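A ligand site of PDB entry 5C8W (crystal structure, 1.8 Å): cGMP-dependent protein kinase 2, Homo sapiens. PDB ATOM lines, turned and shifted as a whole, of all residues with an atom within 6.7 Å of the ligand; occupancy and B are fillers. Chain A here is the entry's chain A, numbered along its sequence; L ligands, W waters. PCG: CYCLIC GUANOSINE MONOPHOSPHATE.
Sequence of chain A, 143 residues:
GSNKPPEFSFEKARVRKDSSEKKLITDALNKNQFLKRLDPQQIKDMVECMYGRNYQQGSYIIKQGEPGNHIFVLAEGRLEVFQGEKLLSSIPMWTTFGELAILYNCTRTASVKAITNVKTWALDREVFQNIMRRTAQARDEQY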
ATOM      1  N   ASN A  32       0.115  12.875   1.298  1.00  0.00           N
ATOM      2  CA  ASN A  32      -0.372  13.895   0.348  1.00  0.00           C
ATOM      3  C   ASN A  32       0.171  15.285   0.713  1.00  0.00           C
ATOM      4  O   ASN A  32       0.122  15.670   1.885  1.00  0.00           O
ATOM      5  CB  ASN A  32      -1.916  13.886   0.302  1.00  0.00           C
ATOM      6  CG  ASN A  32      -2.460  14.887  -0.652  1.00  0.00           C
ATOM      7  OD1 ASN A  32      -2.627  16.066  -0.310  1.00  0.00           O
ATOM      8  ND2 ASN A  32      -2.688  14.457  -1.895  1.00  0.00           N
ATOM      9  N   ILE A  62     -13.743   7.571 -10.999  1.00  0.00           N
ATOM     10  CA  ILE A  62     -13.789   8.985 -11.304  1.00  0.00           C
ATOM     11  C   ILE A  62     -13.837   9.181 -12.831  1.00  0.00           C
ATOM     12  O   ILE A  62     -13.183   8.490 -13.584  1.00  0.00           O
ATOM     13  CB  ILE A  62     -12.569   9.722 -10.705  1.00  0.00           C
ATOM     14  CG1 ILE A  62     -12.713   9.820  -9.196  1.00  0.00           C
ATOM     15  CG2 ILE A  62     -12.387  11.155 -11.339  1.00  0.00           C
ATOM     16  CD1 ILE A  62     -11.456  10.337  -8.500  1.00  0.00           C
ATOM     17  N   GLY A  68     -16.279  16.844  -8.400  1.00  0.00           N
ATOM     18  CA  GLY A  68     -15.807  15.802  -7.474  1.00  0.00           C
ATOM     19  C   GLY A  68     -16.791  15.658  -6.337  1.00  0.00           C
ATOM     20  O   GLY A  68     -17.304  16.673  -5.906  1.00  0.00           O
ATOM     21  N   HIS A  70     -16.113  12.972  -3.758  1.00  0.00           N
ATOM     22  CA  HIS A  70     -15.328  12.236  -2.748  1.00  0.00           C
ATOM     23  C   HIS A  70     -13.848  12.431  -2.848  1.00  0.00           C
ATOM     24  O   HIS A  70     -13.317  12.688  -3.912  1.00  0.00           O
ATOM     25  CB  HIS A  70     -15.591  10.740  -2.874  1.00  0.00           C
ATOM     26  CG  HIS A  70     -17.042  10.395  -2.945  1.00  0.00           C
ATOM     27  ND1 HIS A  70     -17.773  10.436  -4.104  1.00  0.00           N
ATOM     28  CD2 HIS A  70     -17.901  10.020  -1.971  1.00  0.00           C
ATOM     29  CE1 HIS A  70     -19.017  10.100  -3.852  1.00  0.00           C
ATOM     30  NE2 HIS A  70     -19.129   9.850  -2.560  1.00  0.00           N
ATOM     31  N   VAL A  81      -5.038   5.940 -14.376  1.00  0.00           N
ATOM     32  CA  VAL A  81      -5.491   7.309 -14.648  1.00  0.00           C
ATOM     33  C   VAL A  81      -5.378   7.605 -16.146  1.00  0.00           C
ATOM     34  O   VAL A  81      -4.309   7.356 -16.766  1.00  0.00           O
ATOM     35  CB  VAL A  81      -4.669   8.307 -13.834  1.00  0.00           C
ATOM     36  CG1 VAL A  81      -5.183   9.735 -14.037  1.00  0.00           C
ATOM     37  CG2 VAL A  81      -4.695   7.926 -12.366  1.00  0.00           C
ATOM     38  N   GLN A  83      -6.627  10.372 -19.533  1.00  0.00           N
ATOM     39  CA  GLN A  83      -7.279  11.533 -20.131  1.00  0.00           C
ATOM     40  C   GLN A  83      -7.602  11.149 -21.544  1.00  0.00           C
ATOM     41  O   GLN A  83      -6.719  11.015 -22.407  1.00  0.00           O
ATOM     42  CB  GLN A  83      -6.389  12.782 -20.048  1.00  0.00           C
ATOM     43  CG  GLN A  83      -6.288  13.346 -18.617  1.00  0.00           C
ATOM     44  CD  GLN A  83      -5.390  14.564 -18.594  1.00  0.00           C
ATOM     45  OE1 GLN A  83      -4.399  14.639 -19.338  1.00  0.00           O
ATOM     46  NE2 GLN A  83      -5.750  15.529 -17.777  1.00  0.00           N
ATOM     47  N   LEU A  88      -2.029   7.766 -18.240  1.00  0.00           N
ATOM     48  CA  LEU A  88      -1.050   8.616 -17.526  1.00  0.00           C
ATOM     49  C   LEU A  88      -0.253   7.920 -16.430  1.00  0.00           C
ATOM     50  O   LEU A  88       0.928   8.202 -16.274  1.00  0.00           O
ATOM     51  CB  LEU A  88      -1.737   9.818 -16.883  1.00  0.00           C
ATOM     52  CG  LEU A  88      -2.422  10.803 -17.810  1.00  0.00           C
ATOM     53  CD1 LEU A  88      -2.871  11.980 -16.961  1.00  0.00           C
ATOM     54  CD2 LEU A  88      -1.479  11.249 -18.919  1.00  0.00           C
ATOM     55  N   SER A  89      -0.908   7.063 -15.652  1.00  0.00           N
ATOM     56  CA  SER A  89      -0.297   6.514 -14.429  1.00  0.00           C
ATOM     57  C   SER A  89      -1.095   5.434 -13.800  1.00  0.00           C
ATOM     58  O   SER A  89      -2.299   5.293 -14.066  1.00  0.00           O
ATOM     59  CB  SER A  89      -0.079   7.581 -13.342  1.00  0.00           C
ATOM     60  OG  SER A  89      -1.322   8.027 -12.813  1.00  0.00           O
ATOM     61  N   SER A  90      -0.418   4.712 -12.932  1.00  0.00           N
ATOM     62  CA  SER A  90      -1.065   3.746 -12.035  1.00  0.00           C
ATOM     63  C   SER A  90      -0.933   4.289 -10.629  1.00  0.00           C
ATOM     64  O   SER A  90       0.165   4.658 -10.215  1.00  0.00           O
ATOM     65  CB  SER A  90      -0.393   2.359 -12.116  1.00  0.00           C
ATOM     66  OG  SER A  90      -1.090   1.431 -11.295  1.00  0.00           O
ATOM     67  N   ILE A  91      -2.040   4.368  -9.901  1.00  0.00           N
ATOM     68  CA  ILE A  91      -2.025   4.927  -8.563  1.00  0.00           C
ATOM     69  C   ILE A  91      -1.357   3.956  -7.572  1.00  0.00           C
ATOM     70  O   ILE A  91      -1.774   2.799  -7.441  1.00  0.00           O
ATOM     71  CB  ILE A  91      -3.478   5.298  -8.096  1.00  0.00           C
ATOM     72  CG1 ILE A  91      -4.075   6.332  -9.063  1.00  0.00           C
ATOM     73  CG2 ILE A  91      -3.462   5.789  -6.665  1.00  0.00           C
ATOM     74  CD1 ILE A  91      -5.422   6.850  -8.706  1.00  0.00           C
ATOM     75  N   PRO A  92      -0.332   4.417  -6.863  1.00  0.00           N
ATOM     76  CA  PRO A  92       0.331   3.516  -5.922  1.00  0.00           C
ATOM     77  C   PRO A  92      -0.590   3.118  -4.762  1.00  0.00           C
ATOM     78  O   PRO A  92      -1.483   3.882  -4.377  1.00  0.00           O
ATOM     79  CB  PRO A  92       1.504   4.343  -5.408  1.00  0.00           C
ATOM     80  CG  PRO A  92       1.584   5.508  -6.290  1.00  0.00           C
ATOM     81  CD  PRO A  92       0.225   5.777  -6.798  1.00  0.00           C
ATOM     82  N   THR A  96      -3.733   8.651  -1.566  1.00  0.00           N
ATOM     83  CA  THR A  96      -4.938   9.484  -1.698  1.00  0.00           C
ATOM     84  C   THR A  96      -5.139   9.864  -3.152  1.00  0.00           C
ATOM     85  O   THR A  96      -4.169  10.167  -3.852  1.00  0.00           O
ATOM     86  CB  THR A  96      -4.778  10.789  -0.893  1.00  0.00           C
ATOM     87  OG1 THR A  96      -4.452  10.483   0.468  1.00  0.00           O
ATOM     88  CG2 THR A  96      -6.067  11.646  -0.914  1.00  0.00           C
ATOM     89  N   PHE A  97      -6.364   9.875  -3.613  1.00  0.00           N
ATOM     90  CA  PHE A  97      -6.635  10.427  -4.940  1.00  0.00           C
ATOM     91  C   PHE A  97      -8.000  11.055  -4.971  1.00  0.00           C
ATOM     92  O   PHE A  97      -8.823  10.822  -4.089  1.00  0.00           O
ATOM     93  CB  PHE A  97      -6.489   9.362  -6.044  1.00  0.00           C
ATOM     94  CG  PHE A  97      -7.524   8.246  -5.976  1.00  0.00           C
ATOM     95  CD1 PHE A  97      -7.336   7.144  -5.191  1.00  0.00           C
ATOM     96  CD2 PHE A  97      -8.649   8.297  -6.790  1.00  0.00           C
ATOM     97  CE1 PHE A  97      -8.268   6.128  -5.163  1.00  0.00           C
ATOM     98  CE2 PHE A  97      -9.588   7.309  -6.755  1.00  0.00           C
ATOM     99  CZ  PHE A  97      -9.404   6.214  -5.948  1.00  0.00           C
ATOM    100  N   GLY A  98      -8.233  11.865  -5.993  1.00  0.00           N
ATOM    101  CA  GLY A  98      -9.487  12.594  -6.086  1.00  0.00           C
ATOM    102  C   GLY A  98      -9.532  13.835  -5.211  1.00  0.00           C
ATOM    103  O   GLY A  98     -10.603  14.394  -4.970  1.00  0.00           O
ATOM    104  N   GLU A  99      -8.378  14.294  -4.741  1.00  0.00           N
ATOM    105  CA  GLU A  99      -8.356  15.480  -3.905  1.00  0.00           C
ATOM    106  C   GLU A  99      -8.392  16.757  -4.744  1.00  0.00           C
ATOM    107  O   GLU A  99      -8.801  17.797  -4.248  1.00  0.00           O
ATOM    108  CB  GLU A  99      -7.135  15.507  -2.970  1.00  0.00           C
ATOM    109  CG  GLU A  99      -5.816  15.926  -3.586  1.00  0.00           C
ATOM    110  CD  GLU A  99      -5.205  14.922  -4.563  1.00  0.00           C
ATOM    111  OE1 GLU A  99      -5.943  14.291  -5.348  1.00  0.00           O
ATOM    112  OE2 GLU A  99      -3.964  14.826  -4.561  1.00  0.00           O
ATOM    113  N   LEU A 100      -7.955  16.678  -5.994  1.00  0.00           N
ATOM    114  CA  LEU A 100      -7.730  17.930  -6.758  1.00  0.00           C
ATOM    115  C   LEU A 100      -9.014  18.684  -6.983  1.00  0.00           C
ATOM    116  O   LEU A 100      -9.102  19.907  -6.718  1.00  0.00           O
ATOM    117  CB  LEU A 100      -7.081  17.632  -8.100  1.00  0.00           C
ATOM    118  CG  LEU A 100      -5.680  17.012  -8.017  1.00  0.00           C
ATOM    119  CD1 LEU A 100      -5.111  16.924  -9.403  1.00  0.00           C
ATOM    120  CD2 LEU A 100      -4.734  17.788  -7.128  1.00  0.00           C
ATOM    121  N   ALA A 101     -10.024  17.995  -7.495  1.00  0.00           N
ATOM    122  CA  ALA A 101     -11.272  18.667  -7.790  1.00  0.00           C
ATOM    123  C   ALA A 101     -11.903  19.242  -6.535  1.00  0.00           C
ATOM    124  O   ALA A 101     -12.509  20.297  -6.587  1.00  0.00           O
ATOM    125  CB  ALA A 101     -12.288  17.716  -8.479  1.00  0.00           C
ATOM    126  N   ILE A 102     -11.747  18.555  -5.408  1.00  0.00           N
ATOM    127  CA  ILE A 102     -12.307  18.998  -4.131  1.00  0.00           C
ATOM    128  C   ILE A 102     -11.560  20.216  -3.571  1.00  0.00           C
ATOM    129  O   ILE A 102     -12.189  21.171  -3.103  1.00  0.00           O
ATOM    130  CB  ILE A 102     -12.251  17.895  -3.032  1.00  0.00           C
ATOM    131  CG1 ILE A 102     -12.798  16.549  -3.496  1.00  0.00           C
ATOM    132  CG2 ILE A 102     -12.955  18.386  -1.747  1.00  0.00           C
ATOM    133  CD1 ILE A 102     -14.144  16.577  -3.982  1.00  0.00           C
ATOM    134  N   CYS A 106     -12.261  22.774  -9.257  1.00  0.00           N
ATOM    135  CA  CYS A 106     -12.259  22.580 -10.696  1.00  0.00           C
ATOM    136  C   CYS A 106     -12.974  21.247 -10.903  1.00  0.00           C
ATOM    137  O   CYS A 106     -13.201  20.517  -9.946  1.00  0.00           O
ATOM    138  CB  CYS A 106     -10.840  22.543 -11.257  1.00  0.00           C
ATOM    139  SG  CYS A 106      -9.761  21.310 -10.545  1.00  0.00           S
ATOM    140  N   THR A 107     -13.246  20.885 -12.144  1.00  0.00           N
ATOM    141  CA  THR A 107     -13.822  19.567 -12.388  1.00  0.00           C
ATOM    142  C   THR A 107     -12.716  18.518 -12.303  1.00  0.00           C
ATOM    143  O   THR A 107     -11.518  18.847 -12.324  1.00  0.00           O
ATOM    144  CB  THR A 107     -14.532  19.496 -13.754  1.00  0.00           C
ATOM    145  OG1 THR A 107     -13.585  19.693 -14.806  1.00  0.00           O
ATOM    146  CG2 THR A 107     -15.592  20.568 -13.842  1.00  0.00           C
ATOM    147  N   ARG A 108     -13.108  17.248 -12.204  1.00  0.00           N
ATOM    148  CA  ARG A 108     -12.156  16.122 -12.257  1.00  0.00           C
ATOM    149  C   ARG A 108     -11.209  16.267 -13.417  1.00  0.00           C
ATOM    150  O   ARG A 108     -11.642  16.417 -14.571  1.00  0.00           O
ATOM    151  CB  ARG A 108     -12.901  14.777 -12.393  1.00  0.00           C
ATOM    152  CG  ARG A 108     -13.797  14.413 -11.192  1.00  0.00           C
ATOM    153  CD  ARG A 108     -12.945  14.285  -9.925  1.00  0.00           C
ATOM    154  NE  ARG A 108     -13.641  13.539  -8.851  1.00  0.00           N
ATOM    155  CZ  ARG A 108     -13.269  13.519  -7.577  1.00  0.00           C
ATOM    156  NH1 ARG A 108     -12.206  14.184  -7.146  1.00  0.00           N
ATOM    157  NH2 ARG A 108     -13.963  12.797  -6.705  1.00  0.00           N
ATOM    158  N   THR A 109      -9.920  16.252 -13.107  1.00  0.00           N
ATOM    159  CA  THR A 109      -8.912  16.532 -14.124  1.00  0.00           C
ATOM    160  C   THR A 109      -8.640  15.355 -15.075  1.00  0.00           C
ATOM    161  O   THR A 109      -8.034  15.518 -16.143  1.00  0.00           O
ATOM    162  CB  THR A 109      -7.566  16.955 -13.488  1.00  0.00           C
ATOM    163  OG1 THR A 109      -6.959  15.821 -12.831  1.00  0.00           O
ATOM    164  CG2 THR A 109      -7.779  18.063 -12.510  1.00  0.00           C
ATOM    165  N   ALA A 110      -9.105  14.178 -14.680  1.00  0.00           N
ATOM    166  CA  ALA A 110      -8.783  12.930 -15.383  1.00  0.00           C
ATOM    167  C   ALA A 110      -9.723  11.867 -14.909  1.00  0.00           C
ATOM    168  O   ALA A 110     -10.346  12.054 -13.890  1.00  0.00           O
ATOM    169  CB  ALA A 110      -7.335  12.495 -15.121  1.00  0.00           C
ATOM    170  N   SER A 111      -9.800  10.759 -15.640  1.00  0.00           N
ATOM    171  CA  SER A 111     -10.577   9.590 -15.221  1.00  0.00           C
ATOM    172  C   SER A 111      -9.723   8.575 -14.487  1.00  0.00           C
ATOM    173  O   SER A 111      -8.546   8.461 -14.748  1.00  0.00           O
ATOM    174  CB  SER A 111     -11.235   8.913 -16.415  1.00  0.00           C
ATOM    175  OG  SER A 111     -12.076   9.793 -17.121  1.00  0.00           O
ATOM    176  N   VAL A 112     -10.336   7.816 -13.567  1.00  0.00           N
ATOM    177  CA  VAL A 112      -9.632   6.811 -12.808  1.00  0.00           C
ATOM    178  C   VAL A 112     -10.432   5.536 -12.951  1.00  0.00           C
ATOM    179  O   VAL A 112     -11.634   5.512 -12.611  1.00  0.00           O
ATOM    180  CB  VAL A 112      -9.520   7.210 -11.335  1.00  0.00           C
ATOM    181  CG1 VAL A 112      -8.845   6.116 -10.535  1.00  0.00           C
ATOM    182  CG2 VAL A 112      -8.781   8.534 -11.164  1.00  0.00           C
HETATM  183  PA  PCG L   1      -9.009  14.635  -9.497  1.00  0.00           P
HETATM  184  O1A PCG L   1      -8.687  15.359 -10.684  1.00  0.00           O
HETATM  185  O2A PCG L   1      -9.931  15.241  -8.644  1.00  0.00           O
HETATM  186  O5' PCG L   1      -9.550  13.293  -9.932  1.00  0.00           O
HETATM  187  C5' PCG L   1      -8.739  12.429 -10.626  1.00  0.00           C
HETATM  188  C4' PCG L   1      -7.514  12.128  -9.799  1.00  0.00           C
HETATM  189  O4' PCG L   1      -6.552  11.256 -10.247  1.00  0.00           O
HETATM  190  C3' PCG L   1      -6.823  13.413  -9.516  1.00  0.00           C
HETATM  191  O3' PCG L   1      -7.688  14.231  -8.792  1.00  0.00           O
HETATM  192  C2' PCG L   1      -5.559  12.897  -8.864  1.00  0.00           C
HETATM  193  O2' PCG L   1      -5.757  12.682  -7.514  1.00  0.00           O
HETATM  194  C1' PCG L   1      -5.396  11.502  -9.506  1.00  0.00           C
HETATM  195  N9  PCG L   1      -4.174  11.294 -10.295  1.00  0.00           N
HETATM  196  C8  PCG L   1      -3.251  10.385 -10.103  1.00  0.00           C
HETATM  197  N7  PCG L   1      -2.298  10.459 -11.004  1.00  0.00           N
HETATM  198  C5  PCG L   1      -2.621  11.463 -11.804  1.00  0.00           C
HETATM  199  C6  PCG L   1      -2.057  12.082 -12.993  1.00  0.00           C
HETATM  200  O6  PCG L   1      -1.039  11.656 -13.428  1.00  0.00           O
HETATM  201  N1  PCG L   1      -2.717  13.095 -13.514  1.00  0.00           N
HETATM  202  C2  PCG L   1      -3.864  13.562 -13.032  1.00  0.00           C
HETATM  203  N2  PCG L   1      -4.439  14.575 -13.657  1.00  0.00           N
HETATM  204  N3  PCG L   1      -4.464  13.020 -11.961  1.00  0.00           N
HETATM  205  C4  PCG L   1      -3.881  12.003 -11.337  1.00  0.00           C
HETATM  206  O   HOH W   1       1.124  10.788 -11.747  1.00  0.00           O
HETATM  207  O   HOH W   2      -3.201  10.417  -6.666  1.00  0.00           O
HETATM  208  O   HOH W   3       0.733  12.649 -15.344  1.00  0.00           O
HETATM  209  O   HOH W   4      -2.621  13.345  -6.634  1.00  0.00           O
HETATM  210  O   HOH W   5      -0.472   8.376  -9.900  1.00  0.00           O
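Residues that only touch the ligand: Leu 100 (3.5 Å), Phe 97 (3.5 Å), Leu 88 (3.6 Å), Val 112 (3.6 Å), Val 81 (3.6 Å), Ala 110 (3.7 Å) and Ile 62 (3.8 Å). Within 4 Å of the ligand: Ile 62, Val 81, Leu 88, Ser 89, Phe 97, Gly 98, Glu 99, Leu 100, Ala 101, Arg 108, Thr 109, Ala 110 and Val 112. The nearest printed residue that does not touch the ligand is Ile 91 (4.3 Å).
The side-chain carboxylate (OE2) of Glu 99 is in hydrogen-bond range of the side-chain amide nitrogen (ND2) of Asn 32, at 3.0 Å. The side-chain amide nitrogen of Gln 83 lies within hydrogen-bond range of the backbone carbonyl oxygen of Thr 109 (2.8 Å). O of Gly 98 is in hydrogen-bond range of NH1 of Arg 108 (2.7 Å). The guanidinium group of Arg 108 lies within hydrogen-bond range of the backbone carbonyl oxygen of His 70, 2.9 Å away. N of Val 81 is in hydrogen-bond range of O of Ser 89. The backbone NH (N) of Leu 88 is in hydrogen-bond range of the backbone carbonyl oxygen (O) of Val 81, at 2.7 Å. The backbone carbonyl oxygen of Ile 62 sits at hydrogen-bond distance from the backbone NH of Val 112 (2.9 Å).
Water W5 lies within hydrogen-bond range of N7 of the ligand and OG of Ser 89. Water W4 bridges OE2 of Glu 99 (2.9 Å) and O2' of the ligand (3.3 Å).
OE1 of Glu 99 lies within hydrogen-bond range of O2' of the ligand, 2.7 Å away. An oxygen (O1A) of the ligand is in hydrogen-bond range of the backbone NH (N) of Thr 109. The side-chain hydroxyl (OG1) of Thr 109 sits at hydrogen-bond distance from an oxygen (O1A) of the ligand, 2.8 Å away. The guanidinium group (NH1) of Arg 108 is in salt-bridge range of an oxygen (O2A) of the ligand, 2.9 Å away. N of Ala 101 is in hydrogen-bond range of O2A of the ligand, at 3.0 Å. N of Gly 98 is in hydrogen-bond range of O2' of the ligand. A nitrogen (N7) of the ligand is in hydrogen-bond range of the side-chain hydroxyl (OG) of Ser 89 (3.2 Å).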
